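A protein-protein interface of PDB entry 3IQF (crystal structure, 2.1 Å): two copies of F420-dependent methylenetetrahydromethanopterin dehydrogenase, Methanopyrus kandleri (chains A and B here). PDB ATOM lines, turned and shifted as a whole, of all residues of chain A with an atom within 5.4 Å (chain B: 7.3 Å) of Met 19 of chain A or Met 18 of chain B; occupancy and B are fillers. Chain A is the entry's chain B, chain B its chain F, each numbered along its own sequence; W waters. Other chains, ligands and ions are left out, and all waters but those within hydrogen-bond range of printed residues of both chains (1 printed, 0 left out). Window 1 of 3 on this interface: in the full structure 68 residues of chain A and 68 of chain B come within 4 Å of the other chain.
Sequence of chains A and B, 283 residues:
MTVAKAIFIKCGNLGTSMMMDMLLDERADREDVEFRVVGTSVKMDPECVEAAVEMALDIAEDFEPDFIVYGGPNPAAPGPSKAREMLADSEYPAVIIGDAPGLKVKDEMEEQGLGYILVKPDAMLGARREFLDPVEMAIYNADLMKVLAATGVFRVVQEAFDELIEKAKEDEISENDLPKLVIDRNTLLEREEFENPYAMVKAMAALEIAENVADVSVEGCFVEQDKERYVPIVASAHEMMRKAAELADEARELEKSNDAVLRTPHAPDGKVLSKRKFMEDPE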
ATOM      1  N   LYS A  10      -4.399  13.520 -32.922  1.00  0.00           N
ATOM      2  CA  LYS A  10      -5.253  14.462 -32.230  1.00  0.00           C
ATOM      3  C   LYS A  10      -6.090  15.254 -33.213  1.00  0.00           C
ATOM      4  O   LYS A  10      -5.562  16.024 -34.000  1.00  0.00           O
ATOM      5  CB  LYS A  10      -4.430  15.408 -31.383  1.00  0.00           C
ATOM      6  CG  LYS A  10      -3.529  14.702 -30.384  1.00  0.00           C
ATOM      7  CD  LYS A  10      -2.966  15.661 -29.344  1.00  0.00           C
ATOM      8  CE  LYS A  10      -1.849  14.947 -28.510  1.00  0.00           C
ATOM      9  NZ  LYS A  10      -1.329  15.813 -27.465  1.00  0.00           N
ATOM     10  N   LEU A  14      -9.869  17.433 -26.489  1.00  0.00           N
ATOM     11  CA  LEU A  14     -10.341  17.024 -25.184  1.00  0.00           C
ATOM     12  C   LEU A  14      -9.229  17.328 -24.190  1.00  0.00           C
ATOM     13  O   LEU A  14      -8.081  17.393 -24.581  1.00  0.00           O
ATOM     14  CB  LEU A  14     -10.569  15.534 -25.209  1.00  0.00           C
ATOM     15  CG  LEU A  14     -11.959  14.948 -25.191  1.00  0.00           C
ATOM     16  CD1 LEU A  14     -13.108  15.904 -25.533  1.00  0.00           C
ATOM     17  CD2 LEU A  14     -11.956  13.672 -25.907  1.00  0.00           C
ATOM     18  N   GLY A  15      -9.568  17.523 -22.907  1.00  0.00           N
ATOM     19  CA  GLY A  15      -8.520  17.651 -21.860  1.00  0.00           C
ATOM     20  C   GLY A  15      -7.557  16.464 -21.862  1.00  0.00           C
ATOM     21  O   GLY A  15      -6.322  16.643 -21.814  1.00  0.00           O
ATOM     22  N   THR A  16      -8.121  15.263 -22.025  1.00  0.00           N
ATOM     23  CA  THR A  16      -7.318  14.053 -22.011  1.00  0.00           C
ATOM     24  C   THR A  16      -6.459  13.916 -23.241  1.00  0.00           C
ATOM     25  O   THR A  16      -5.313  13.517 -23.157  1.00  0.00           O
ATOM     26  CB  THR A  16      -8.196  12.833 -21.788  1.00  0.00           C
ATOM     27  OG1 THR A  16      -8.923  13.038 -20.559  1.00  0.00           O
ATOM     28  CG2 THR A  16      -7.365  11.576 -21.712  1.00  0.00           C
ATOM     29  N   SER A  17      -6.992  14.266 -24.400  1.00  0.00           N
ATOM     30  CA  SER A  17      -6.243  14.096 -25.632  1.00  0.00           C
ATOM     31  C   SER A  17      -5.118  15.094 -25.736  1.00  0.00           C
ATOM     32  O   SER A  17      -4.085  14.830 -26.340  1.00  0.00           O
ATOM     33  CB  SER A  17      -7.179  14.216 -26.852  1.00  0.00           C
ATOM     34  OG  SER A  17      -7.780  15.521 -26.965  1.00  0.00           O
ATOM     35  N   MET A  18      -5.329  16.261 -25.147  1.00  0.00           N
ATOM     36  CA  MET A  18      -4.310  17.304 -25.148  1.00  0.00           C
ATOM     37  C   MET A  18      -3.071  16.888 -24.349  1.00  0.00           C
ATOM     38  O   MET A  18      -1.963  17.176 -24.717  1.00  0.00           O
ATOM     39  CB  MET A  18      -4.904  18.582 -24.587  1.00  0.00           C
ATOM     40  CG  MET A  18      -4.134  19.843 -24.865  1.00  0.00           C
ATOM     41  SD  MET A  18      -5.049  21.313 -24.239  1.00  0.00           S
ATOM     42  CE  MET A  18      -3.984  22.598 -24.756  1.00  0.00           C
ATOM     43  N   MET A  19      -3.269  16.184 -23.247  1.00  0.00           N
ATOM     44  CA  MET A  19      -2.189  15.841 -22.337  1.00  0.00           C
ATOM     45  C   MET A  19      -1.688  14.415 -22.478  1.00  0.00           C
ATOM     46  O   MET A  19      -0.632  14.100 -21.955  1.00  0.00           O
ATOM     47  CB  MET A  19      -2.708  16.089 -20.912  1.00  0.00           C
ATOM     48  CG  MET A  19      -2.418  17.558 -20.492  1.00  0.00           C
ATOM     49  SD  MET A  19      -0.664  17.865 -19.963  1.00  0.00           S
ATOM     50  CE  MET A  19      -0.491  16.388 -19.035  1.00  0.00           C
ATOM     51  N   MET A  20      -2.429  13.553 -23.191  1.00  0.00           N
ATOM     52  CA  MET A  20      -2.209  12.108 -23.099  1.00  0.00           C
ATOM     53  C   MET A  20      -0.756  11.652 -23.331  1.00  0.00           C
ATOM     54  O   MET A  20      -0.231  10.843 -22.567  1.00  0.00           O
ATOM     55  CB  MET A  20      -3.158  11.349 -24.036  1.00  0.00           C
ATOM     56  CG  MET A  20      -2.994  11.639 -25.504  1.00  0.00           C
ATOM     57  SD  MET A  20      -4.274  10.840 -26.507  1.00  0.00           S
ATOM     58  CE  MET A  20      -4.165  11.697 -28.069  1.00  0.00           C
ATOM     59  N   ASP A  21      -0.097  12.123 -24.375  1.00  0.00           N
ATOM     60  CA  ASP A  21       1.311  11.713 -24.624  1.00  0.00           C
ATOM     61  C   ASP A  21       2.285  12.246 -23.527  1.00  0.00           C
ATOM     62  O   ASP A  21       3.240  11.567 -23.115  1.00  0.00           O
ATOM     63  CB  ASP A  21       1.745  12.122 -26.026  1.00  0.00           C
ATOM     64  CG  ASP A  21       1.530  13.553 -26.307  1.00  0.00           C
ATOM     65  OD1 ASP A  21       0.352  14.017 -26.270  1.00  0.00           O
ATOM     66  OD2 ASP A  21       2.532  14.253 -26.543  1.00  0.00           O
ATOM     67  N   MET A  22       2.015  13.452 -23.023  1.00  0.00           N
ATOM     68  CA  MET A  22       2.931  14.086 -22.104  1.00  0.00           C
ATOM     69  C   MET A  22       2.896  13.504 -20.715  1.00  0.00           C
ATOM     70  O   MET A  22       3.892  13.582 -19.999  1.00  0.00           O
ATOM     71  CB  MET A  22       2.675  15.583 -22.058  1.00  0.00           C
ATOM     72  CG  MET A  22       2.899  16.167 -23.448  1.00  0.00           C
ATOM     73  SD  MET A  22       3.036  17.929 -23.363  1.00  0.00           S
ATOM     74  CE  MET A  22       1.325  18.389 -23.089  1.00  0.00           C
ATOM     75  N   LEU A  23       1.760  12.925 -20.344  1.00  0.00           N
ATOM     76  CA  LEU A  23       1.622  12.201 -19.095  1.00  0.00           C
ATOM     77  C   LEU A  23       2.537  10.979 -19.021  1.00  0.00           C
ATOM     78  O   LEU A  23       2.758  10.441 -17.956  1.00  0.00           O
ATOM     79  CB  LEU A  23       0.175  11.727 -18.889  1.00  0.00           C
ATOM     80  CG  LEU A  23      -0.891  12.800 -18.717  1.00  0.00           C
ATOM     81  CD1 LEU A  23      -2.253  12.164 -18.814  1.00  0.00           C
ATOM     82  CD2 LEU A  23      -0.737  13.558 -17.438  1.00  0.00           C
ATOM     83  N   MET A 145      -8.269  20.845 -17.002  1.00  0.00           N
ATOM     84  CA  MET A 145      -7.004  20.166 -16.786  1.00  0.00           C
ATOM     85  C   MET A 145      -6.686  20.013 -15.300  1.00  0.00           C
ATOM     86  O   MET A 145      -6.213  18.985 -14.822  1.00  0.00           O
ATOM     87  CB  MET A 145      -5.896  20.970 -17.431  1.00  0.00           C
ATOM     88  CG  MET A 145      -4.587  20.189 -17.546  1.00  0.00           C
ATOM     89  SD  MET A 145      -3.296  21.212 -18.236  1.00  0.00           S
ATOM     90  CE  MET A 145      -3.720  21.159 -19.949  1.00  0.00           C
ATOM     91  N   PHE A 154      -5.947  11.670 -14.557  1.00  0.00           N
ATOM     92  CA  PHE A 154      -4.776  11.543 -15.422  1.00  0.00           C
ATOM     93  C   PHE A 154      -3.865  10.413 -14.991  1.00  0.00           C
ATOM     94  O   PHE A 154      -3.179   9.878 -15.799  1.00  0.00           O
ATOM     95  CB  PHE A 154      -3.985  12.823 -15.496  1.00  0.00           C
ATOM     96  CG  PHE A 154      -4.563  13.861 -16.414  1.00  0.00           C
ATOM     97  CD1 PHE A 154      -4.162  15.149 -16.318  1.00  0.00           C
ATOM     98  CD2 PHE A 154      -5.510  13.546 -17.383  1.00  0.00           C
ATOM     99  CE1 PHE A 154      -4.666  16.150 -17.198  1.00  0.00           C
ATOM    100  CE2 PHE A 154      -6.025  14.520 -18.199  1.00  0.00           C
ATOM    101  CZ  PHE A 154      -5.598  15.815 -18.127  1.00  0.00           C
ATOM    102  N   LYS B  10       5.465  20.898 -32.808  1.00  0.00           N
ATOM    103  CA  LYS B  10       5.548  20.969 -31.371  1.00  0.00           C
ATOM    104  C   LYS B  10       6.592  19.973 -30.849  1.00  0.00           C
ATOM    105  O   LYS B  10       6.388  18.769 -30.932  1.00  0.00           O
ATOM    106  CB  LYS B  10       4.165  20.661 -30.805  1.00  0.00           C
ATOM    107  CG  LYS B  10       3.013  21.638 -31.300  1.00  0.00           C
ATOM    108  CD  LYS B  10       1.648  21.372 -30.645  1.00  0.00           C
ATOM    109  CE  LYS B  10       0.635  22.392 -31.112  1.00  0.00           C
ATOM    110  NZ  LYS B  10      -0.594  22.376 -30.262  1.00  0.00           N
ATOM    111  N   GLY B  12       8.784  19.373 -27.195  1.00  0.00           N
ATOM    112  CA  GLY B  12       8.851  19.862 -25.829  1.00  0.00           C
ATOM    113  C   GLY B  12       7.500  20.475 -25.568  1.00  0.00           C
ATOM    114  O   GLY B  12       6.608  20.341 -26.400  1.00  0.00           O
ATOM    115  N   ASN B  13       7.339  21.170 -24.445  1.00  0.00           N
ATOM    116  CA  ASN B  13       6.074  21.773 -24.125  1.00  0.00           C
ATOM    117  C   ASN B  13       6.229  23.127 -23.480  1.00  0.00           C
ATOM    118  O   ASN B  13       7.013  23.299 -22.550  1.00  0.00           O
ATOM    119  CB  ASN B  13       5.201  20.848 -23.236  1.00  0.00           C
ATOM    120  CG  ASN B  13       3.792  21.360 -23.128  1.00  0.00           C
ATOM    121  OD1 ASN B  13       3.120  21.553 -24.156  1.00  0.00           O
ATOM    122  ND2 ASN B  13       3.361  21.698 -21.897  1.00  0.00           N
ATOM    123  N   LEU B  14       5.457  24.080 -23.994  1.00  0.00           N
ATOM    124  CA  LEU B  14       5.226  25.362 -23.330  1.00  0.00           C
ATOM    125  C   LEU B  14       3.741  25.570 -23.258  1.00  0.00           C
ATOM    126  O   LEU B  14       3.009  25.035 -24.080  1.00  0.00           O
ATOM    127  CB  LEU B  14       5.814  26.481 -24.174  1.00  0.00           C
ATOM    128  CG  LEU B  14       7.123  27.191 -23.851  1.00  0.00           C
ATOM    129  CD1 LEU B  14       8.130  26.472 -22.982  1.00  0.00           C
ATOM    130  CD2 LEU B  14       7.686  27.668 -25.145  1.00  0.00           C
ATOM    131  N   GLY B  15       3.273  26.409 -22.368  1.00  0.00           N
ATOM    132  CA  GLY B  15       1.840  26.800 -22.377  1.00  0.00           C
ATOM    133  C   GLY B  15       1.360  27.359 -23.727  1.00  0.00           C
ATOM    134  O   GLY B  15       0.305  26.961 -24.277  1.00  0.00           O
ATOM    135  N   THR B  16       2.193  28.196 -24.318  1.00  0.00           N
ATOM    136  CA  THR B  16       1.853  28.858 -25.589  1.00  0.00           C
ATOM    137  C   THR B  16       1.856  27.883 -26.754  1.00  0.00           C
ATOM    138  O   THR B  16       0.917  27.886 -27.565  1.00  0.00           O
ATOM    139  CB  THR B  16       2.813  29.989 -25.859  1.00  0.00           C
ATOM    140  OG1 THR B  16       2.765  30.897 -24.740  1.00  0.00           O
ATOM    141  CG2 THR B  16       2.418  30.730 -27.140  1.00  0.00           C
ATOM    142  N   SER B  17       2.852  27.005 -26.813  1.00  0.00           N
ATOM    143  CA  SER B  17       2.952  26.090 -27.915  1.00  0.00           C
ATOM    144  C   SER B  17       1.837  25.042 -27.824  1.00  0.00           C
ATOM    145  O   SER B  17       1.330  24.598 -28.824  1.00  0.00           O
ATOM    146  CB  SER B  17       4.366  25.504 -28.059  1.00  0.00           C
ATOM    147  OG  SER B  17       4.656  24.574 -27.041  1.00  0.00           O
ATOM    148  N   MET B  18       1.400  24.720 -26.625  1.00  0.00           N
ATOM    149  CA  MET B  18       0.344  23.755 -26.424  1.00  0.00           C
ATOM    150  C   MET B  18      -0.979  24.239 -27.005  1.00  0.00           C
ATOM    151  O   MET B  18      -1.721  23.463 -27.587  1.00  0.00           O
ATOM    152  CB  MET B  18       0.204  23.509 -24.927  1.00  0.00           C
ATOM    153  CG  MET B  18      -0.501  22.242 -24.562  1.00  0.00           C
ATOM    154  SD  MET B  18      -0.428  22.041 -22.746  1.00  0.00           S
ATOM    155  CE  MET B  18      -1.415  20.615 -22.637  1.00  0.00           C
ATOM    156  N   MET B  19      -1.236  25.531 -26.883  1.00  0.00           N
ATOM    157  CA  MET B  19      -2.530  26.122 -27.256  1.00  0.00           C
ATOM    158  C   MET B  19      -2.526  26.836 -28.601  1.00  0.00           C
ATOM    159  O   MET B  19      -3.597  27.174 -29.105  1.00  0.00           O
ATOM    160  CB  MET B  19      -2.955  27.114 -26.156  1.00  0.00           C
ATOM    161  CG  MET B  19      -3.639  26.402 -24.993  1.00  0.00           C
ATOM    162  SD  MET B  19      -5.391  26.012 -25.419  1.00  0.00           S
ATOM    163  CE  MET B  19      -5.877  27.499 -26.187  1.00  0.00           C
ATOM    164  N   MET B  20      -1.351  27.087 -29.154  1.00  0.00           N
ATOM    165  CA  MET B  20      -1.210  28.119 -30.199  1.00  0.00           C
ATOM    166  C   MET B  20      -2.144  27.946 -31.397  1.00  0.00           C
ATOM    167  O   MET B  20      -2.751  28.918 -31.835  1.00  0.00           O
ATOM    168  CB  MET B  20       0.236  28.243 -30.709  1.00  0.00           C
ATOM    169  CG  MET B  20       0.877  26.915 -31.129  1.00  0.00           C
ATOM    170  SD  MET B  20       2.613  27.255 -31.504  1.00  0.00           S
ATOM    171  CE  MET B  20       3.190  25.637 -32.004  1.00  0.00           C
ATOM    172  N   ASP B  21      -2.242  26.739 -31.933  1.00  0.00           N
ATOM    173  CA  ASP B  21      -3.131  26.464 -33.074  1.00  0.00           C
ATOM    174  C   ASP B  21      -4.627  26.615 -32.701  1.00  0.00           C
ATOM    175  O   ASP B  21      -5.413  27.223 -33.433  1.00  0.00           O
ATOM    176  CB  ASP B  21      -2.824  25.101 -33.683  1.00  0.00           C
ATOM    177  CG  ASP B  21      -2.842  23.974 -32.652  1.00  0.00           C
ATOM    178  OD1 ASP B  21      -2.099  24.022 -31.650  1.00  0.00           O
ATOM    179  OD2 ASP B  21      -3.643  23.049 -32.806  1.00  0.00           O
ATOM    180  N   MET B  22      -5.004  26.138 -31.526  1.00  0.00           N
ATOM    181  CA  MET B  22      -6.392  26.141 -31.111  1.00  0.00           C
ATOM    182  C   MET B  22      -6.942  27.532 -30.835  1.00  0.00           C
ATOM    183  O   MET B  22      -8.124  27.781 -31.027  1.00  0.00           O
ATOM    184  CB  MET B  22      -6.546  25.275 -29.858  1.00  0.00           C
ATOM    185  CG  MET B  22      -6.132  23.845 -30.145  1.00  0.00           C
ATOM    186  SD  MET B  22      -6.451  22.643 -28.850  1.00  0.00           S
ATOM    187  CE  MET B  22      -5.233  23.196 -27.684  1.00  0.00           C
ATOM    188  N   LEU B  23      -6.074  28.450 -30.423  1.00  0.00           N
ATOM    189  CA  LEU B  23      -6.436  29.863 -30.236  1.00  0.00           C
ATOM    190  C   LEU B  23      -6.905  30.542 -31.537  1.00  0.00           C
ATOM    191  O   LEU B  23      -7.555  31.578 -31.502  1.00  0.00           O
ATOM    192  CB  LEU B  23      -5.243  30.642 -29.698  1.00  0.00           C
ATOM    193  CG  LEU B  23      -4.702  30.247 -28.321  1.00  0.00           C
ATOM    194  CD1 LEU B  23      -3.345  30.925 -28.092  1.00  0.00           C
ATOM    195  CD2 LEU B  23      -5.716  30.556 -27.251  1.00  0.00           C
ATOM    196  N   SER B  41       6.261  14.961 -29.302  1.00  0.00           N
ATOM    197  CA  SER B  41       5.850  15.045 -27.934  1.00  0.00           C
ATOM    198  C   SER B  41       6.861  15.909 -27.144  1.00  0.00           C
ATOM    199  O   SER B  41       7.341  16.946 -27.645  1.00  0.00           O
ATOM    200  CB  SER B  41       5.658  13.608 -27.369  1.00  0.00           C
ATOM    201  OG  SER B  41       4.903  13.658 -26.171  1.00  0.00           O
ATOM    202  N   GLY B  71       7.160  25.495 -32.206  1.00  0.00           N
ATOM    203  CA  GLY B  71       6.920  25.925 -30.852  1.00  0.00           C
ATOM    204  C   GLY B  71       7.461  24.969 -29.811  1.00  0.00           C
ATOM    205  O   GLY B  71       7.297  23.747 -29.926  1.00  0.00           O
ATOM    206  N   GLY B  72       8.115  25.537 -28.799  1.00  0.00           N
ATOM    207  CA  GLY B  72       8.567  24.762 -27.663  1.00  0.00           C
ATOM    208  C   GLY B  72       9.597  25.521 -26.888  1.00  0.00           C
ATOM    209  O   GLY B  72       9.954  26.648 -27.240  1.00  0.00           O
ATOM    210  N   ILE B  97       7.950  30.007 -31.711  1.00  0.00           N
ATOM    211  CA  ILE B  97       7.311  30.267 -30.434  1.00  0.00           C
ATOM    212  C   ILE B  97       8.215  29.711 -29.350  1.00  0.00           C
ATOM    213  O   ILE B  97       8.586  28.523 -29.400  1.00  0.00           O
ATOM    214  CB  ILE B  97       5.946  29.572 -30.276  1.00  0.00           C
ATOM    215  CG1 ILE B  97       4.903  30.100 -31.245  1.00  0.00           C
ATOM    216  CG2 ILE B  97       5.415  29.726 -28.837  1.00  0.00           C
ATOM    217  CD1 ILE B  97       5.114  31.498 -31.729  1.00  0.00           C
ATOM    218  N   ASP B 122       6.039  32.306 -19.822  1.00  0.00           N
ATOM    219  CA  ASP B 122       5.840  30.875 -20.144  1.00  0.00           C
ATOM    220  C   ASP B 122       7.005  30.105 -19.498  1.00  0.00           C
ATOM    221  O   ASP B 122       7.912  29.601 -20.171  1.00  0.00           O
ATOM    222  CB  ASP B 122       5.779  30.658 -21.645  1.00  0.00           C
ATOM    223  CG  ASP B 122       4.943  29.442 -22.032  1.00  0.00           C
ATOM    224  OD1 ASP B 122       4.900  28.453 -21.250  1.00  0.00           O
ATOM    225  OD2 ASP B 122       4.310  29.487 -23.123  1.00  0.00           O
ATOM    226  N   PRO B 134       3.607  13.013 -13.598  1.00  0.00           N
ATOM    227  CA  PRO B 134       2.666  13.462 -14.601  1.00  0.00           C
ATOM    228  C   PRO B 134       1.556  14.385 -14.079  1.00  0.00           C
ATOM    229  O   PRO B 134       1.276  15.438 -14.687  1.00  0.00           O
ATOM    230  CB  PRO B 134       2.099  12.137 -15.122  1.00  0.00           C
ATOM    231  CG  PRO B 134       3.279  11.234 -15.029  1.00  0.00           C
ATOM    232  CD  PRO B 134       3.827  11.558 -13.662  1.00  0.00           C
ATOM    233  N   VAL B 135       0.952  14.015 -12.947  1.00  0.00           N
ATOM    234  CA  VAL B 135      -0.090  14.851 -12.356  1.00  0.00           C
ATOM    235  C   VAL B 135       0.388  16.273 -11.993  1.00  0.00           C
ATOM    236  O   VAL B 135      -0.296  17.254 -12.313  1.00  0.00           O
ATOM    237  CB  VAL B 135      -0.760  14.144 -11.155  1.00  0.00           C
ATOM    238  CG1 VAL B 135      -1.543  15.117 -10.324  1.00  0.00           C
ATOM    239  CG2 VAL B 135      -1.679  13.036 -11.696  1.00  0.00           C
ATOM    240  N   MET B 137       2.932  17.864 -13.245  1.00  0.00           N
ATOM    241  CA  MET B 137       3.189  18.497 -14.532  1.00  0.00           C
ATOM    242  C   MET B 137       1.896  19.075 -15.122  1.00  0.00           C
ATOM    243  O   MET B 137       1.896  20.200 -15.626  1.00  0.00           O
ATOM    244  CB  MET B 137       3.863  17.482 -15.492  1.00  0.00           C
ATOM    245  CG  MET B 137       4.215  18.001 -16.877  1.00  0.00           C
ATOM    246  SD  MET B 137       2.796  17.841 -17.964  1.00  0.00           S
ATOM    247  CE  MET B 137       2.668  16.056 -18.084  1.00  0.00           C
ATOM    248  N   ALA B 138       0.795  18.320 -15.034  1.00  0.00           N
ATOM    249  CA  ALA B 138      -0.464  18.768 -15.567  1.00  0.00           C
ATOM    250  C   ALA B 138      -1.107  19.897 -14.734  1.00  0.00           C
ATOM    251  O   ALA B 138      -1.664  20.849 -15.274  1.00  0.00           O
ATOM    252  CB  ALA B 138      -1.377  17.582 -15.693  1.00  0.00           C
ATOM    253  N   ILE B 139      -1.014  19.769 -13.408  1.00  0.00           N
ATOM    254  CA  ILE B 139      -1.419  20.835 -12.483  1.00  0.00           C
ATOM    255  C   ILE B 139      -0.724  22.165 -12.813  1.00  0.00           C
ATOM    256  O   ILE B 139      -1.385  23.185 -12.929  1.00  0.00           O
ATOM    257  CB  ILE B 139      -1.167  20.426 -11.060  1.00  0.00           C
ATOM    258  CG1 ILE B 139      -2.167  19.307 -10.682  1.00  0.00           C
ATOM    259  CG2 ILE B 139      -1.310  21.660 -10.070  1.00  0.00           C
ATOM    260  CD1 ILE B 139      -2.079  18.821  -9.358  1.00  0.00           C
ATOM    261  N   ASN B 141       0.691  23.056 -15.647  1.00  0.00           N
ATOM    262  CA  ASN B 141       0.186  23.491 -16.931  1.00  0.00           C
ATOM    263  C   ASN B 141      -1.194  24.118 -16.848  1.00  0.00           C
ATOM    264  O   ASN B 141      -1.485  25.035 -17.599  1.00  0.00           O
ATOM    265  CB  ASN B 141       0.224  22.340 -17.916  1.00  0.00           C
ATOM    266  CG  ASN B 141       1.571  22.243 -18.586  1.00  0.00           C
ATOM    267  OD1 ASN B 141       1.845  23.012 -19.510  1.00  0.00           O
ATOM    268  ND2 ASN B 141       2.470  21.451 -18.022  1.00  0.00           N
ATOM    269  N   ALA B 142      -2.053  23.602 -15.973  1.00  0.00           N
ATOM    270  CA  ALA B 142      -3.371  24.180 -15.784  1.00  0.00           C
ATOM    271  C   ALA B 142      -3.262  25.601 -15.250  1.00  0.00           C
ATOM    272  O   ALA B 142      -3.990  26.492 -15.701  1.00  0.00           O
ATOM    273  CB  ALA B 142      -4.230  23.320 -14.816  1.00  0.00           C
ATOM    274  N   MET B 145      -1.794  27.917 -17.918  1.00  0.00           N
ATOM    275  CA  MET B 145      -2.711  28.186 -18.966  1.00  0.00           C
ATOM    276  C   MET B 145      -3.725  29.230 -18.527  1.00  0.00           C
ATOM    277  O   MET B 145      -4.121  30.118 -19.328  1.00  0.00           O
ATOM    278  CB  MET B 145      -3.407  26.870 -19.392  1.00  0.00           C
ATOM    279  CG  MET B 145      -4.401  27.075 -20.522  1.00  0.00           C
ATOM    280  SD  MET B 145      -5.111  25.483 -20.996  1.00  0.00           S
ATOM    281  CE  MET B 145      -3.697  24.606 -21.599  1.00  0.00           C
ATOM    282  N   PHE B 154      -2.608  35.190 -24.340  1.00  0.00           N
ATOM    283  CA  PHE B 154      -3.051  34.378 -25.480  1.00  0.00           C
ATOM    284  C   PHE B 154      -3.759  35.231 -26.543  1.00  0.00           C
ATOM    285  O   PHE B 154      -3.734  34.876 -27.742  1.00  0.00           O
ATOM    286  CB  PHE B 154      -3.945  33.218 -25.056  1.00  0.00           C
ATOM    287  CG  PHE B 154      -3.201  32.002 -24.484  1.00  0.00           C
ATOM    288  CD1 PHE B 154      -3.887  31.071 -23.729  1.00  0.00           C
ATOM    289  CD2 PHE B 154      -1.844  31.785 -24.702  1.00  0.00           C
ATOM    290  CE1 PHE B 154      -3.226  29.929 -23.212  1.00  0.00           C
ATOM    291  CE2 PHE B 154      -1.191  30.673 -24.175  1.00  0.00           C
ATOM    292  CZ  PHE B 154      -1.886  29.744 -23.445  1.00  0.00           C
HETATM  293  O   HOH W   1       5.619  12.187 -24.156  1.00  0.00           O
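The backbone NH (N) of Ala 142 of chain B lies within hydrogen-bond range of the side-chain sulfur (SD) of Met 145 of chain A, at 3.5 Å. OD2 of Asp 21 of chain A sits at hydrogen-bond distance from OG of Ser 41 of chain B, at 2.5 Å. The side-chain amide oxygen (OD1) of Asn 13 of chain B sits close to the side-chain sulfur (SD) of Met 22 of chain A (3.7 Å). The side-chain sulfur (SD) of Met 145 of chain A sits close to the backbone carbonyl oxygen (O) of Ala 138 of chain B (3.4 Å).
ND2 of Asn 13 of chain B lies within hydrogen-bond range of OD1 of Asn 141 of chain B (3.1 Å). The backbone carbonyl oxygen (O) of Met 18 of chain B is in hydrogen-bond range of the side-chain amino group (NZ) of Lys 10 of chain B. The side-chain amino group (NZ) of Lys 10 of chain A is in salt-bridge range of the side-chain carboxylate (OD1) of Asp 21 of chain A (2.7 Å). The side-chain amino group (NZ) of Lys 10 of chain A sits at hydrogen-bond distance from the backbone carbonyl oxygen (O) of Met 18 of chain A (3.1 Å). O of Met 137 of chain B lies within hydrogen-bond range of ND2 of Asn 141 of chain B (2.8 Å).
Among the printed residues, pairs that only touch across the chains: Met 18 of chain A with Met 18 of chain B, Met 18 of chain A with Met 19 of chain B, Met 18 of chain A with Met 22 of chain B, Met 18 of chain A with Met 145 of chain B, Met 19 of chain A with Met 18 of chain B, Met 19 of chain A with Met 137 of chain B, Met 19 of chain A with Ala 138 of chain B, Met 22 of chain A with Met 18 of chain B, Met 22 of chain A with Met 137 of chain B, Leu 23 of chain A with Pro 134 of chain B, Leu 23 of chain A with Met 137 of chain B, Met 145 of chain A with Met 18 of chain B, Met 145 of chain A with Asn 141 of chain B, Met 145 of chain A with Met 145 of chain B and Phe 154 of chain A with Ala 138 of chain B.
Of the printed residues of chain B, Met 19 of chain A touches Met 18 (3.9 Å), Met 137 (3.3 Å) and Ala 138 (3.7 Å). Printed residues of chain B within 4 Å of Asp 21 of chain A: Ser 41 (2.5 Å). Of the printed residues of chain B, Phe 154 of chain A touches Ala 138 (3.8 Å). Printed residues of chain A within 4 Å of Asn 13 of chain B: Met 22. Of the printed residues of chain B, Leu 23 of chain A touches Pro 134 and Met 137. Of the printed residues of chain B, Met 145 of chain A touches Met 18, Ala 138, Asn 141, Ala 142 and Met 145. Leu 23 of chain B touches none of the printed residues of chain A. The nearest residue of chain B that does not touch Met 19 of chain A is Pro 134 of chain B (4.8 Å).
Of the 27 printed residues of chain B, 11 touch a printed residue of chain A. Printed residues of chain B that touch a printed residue of chain A: Asn 13, Met 18, Met 19, Met 22, Ser 41, Pro 134, Met 137, Ala 138, Asn 141, Ala 142 and Met 145. Hydrophobic or aromatic side chains of chain A that line the printed part of chain B: Met 18, Met 19, Met 22, Leu 23, Met 145 and Phe 154.
Met 18 of chain A touches its own counterpart, Met 18 of chain B. Met 18 of chain A touches Met 19 of chain B, and with the chains exchanged Met 19 of chain A touches Met 18 of chain B. Met 18 of chain A touches Met 145 of chain B, and with the chains exchanged Met 145 of chain A touches Met 18 of chain B. Met 145 of chain B touches its own counterpart, Met 145 of chain A. Of the 19 pairs that touch across the chains among the printed residues, 8 have their exchanged pair printed and touching as well.
Water W1 lies within hydrogen-bond range of the side-chain hydroxyl of Ser 41 of chain B (2.6 Å) and the backbone carbonyl oxygen of Asp 21 of chain A (2.7 Å).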
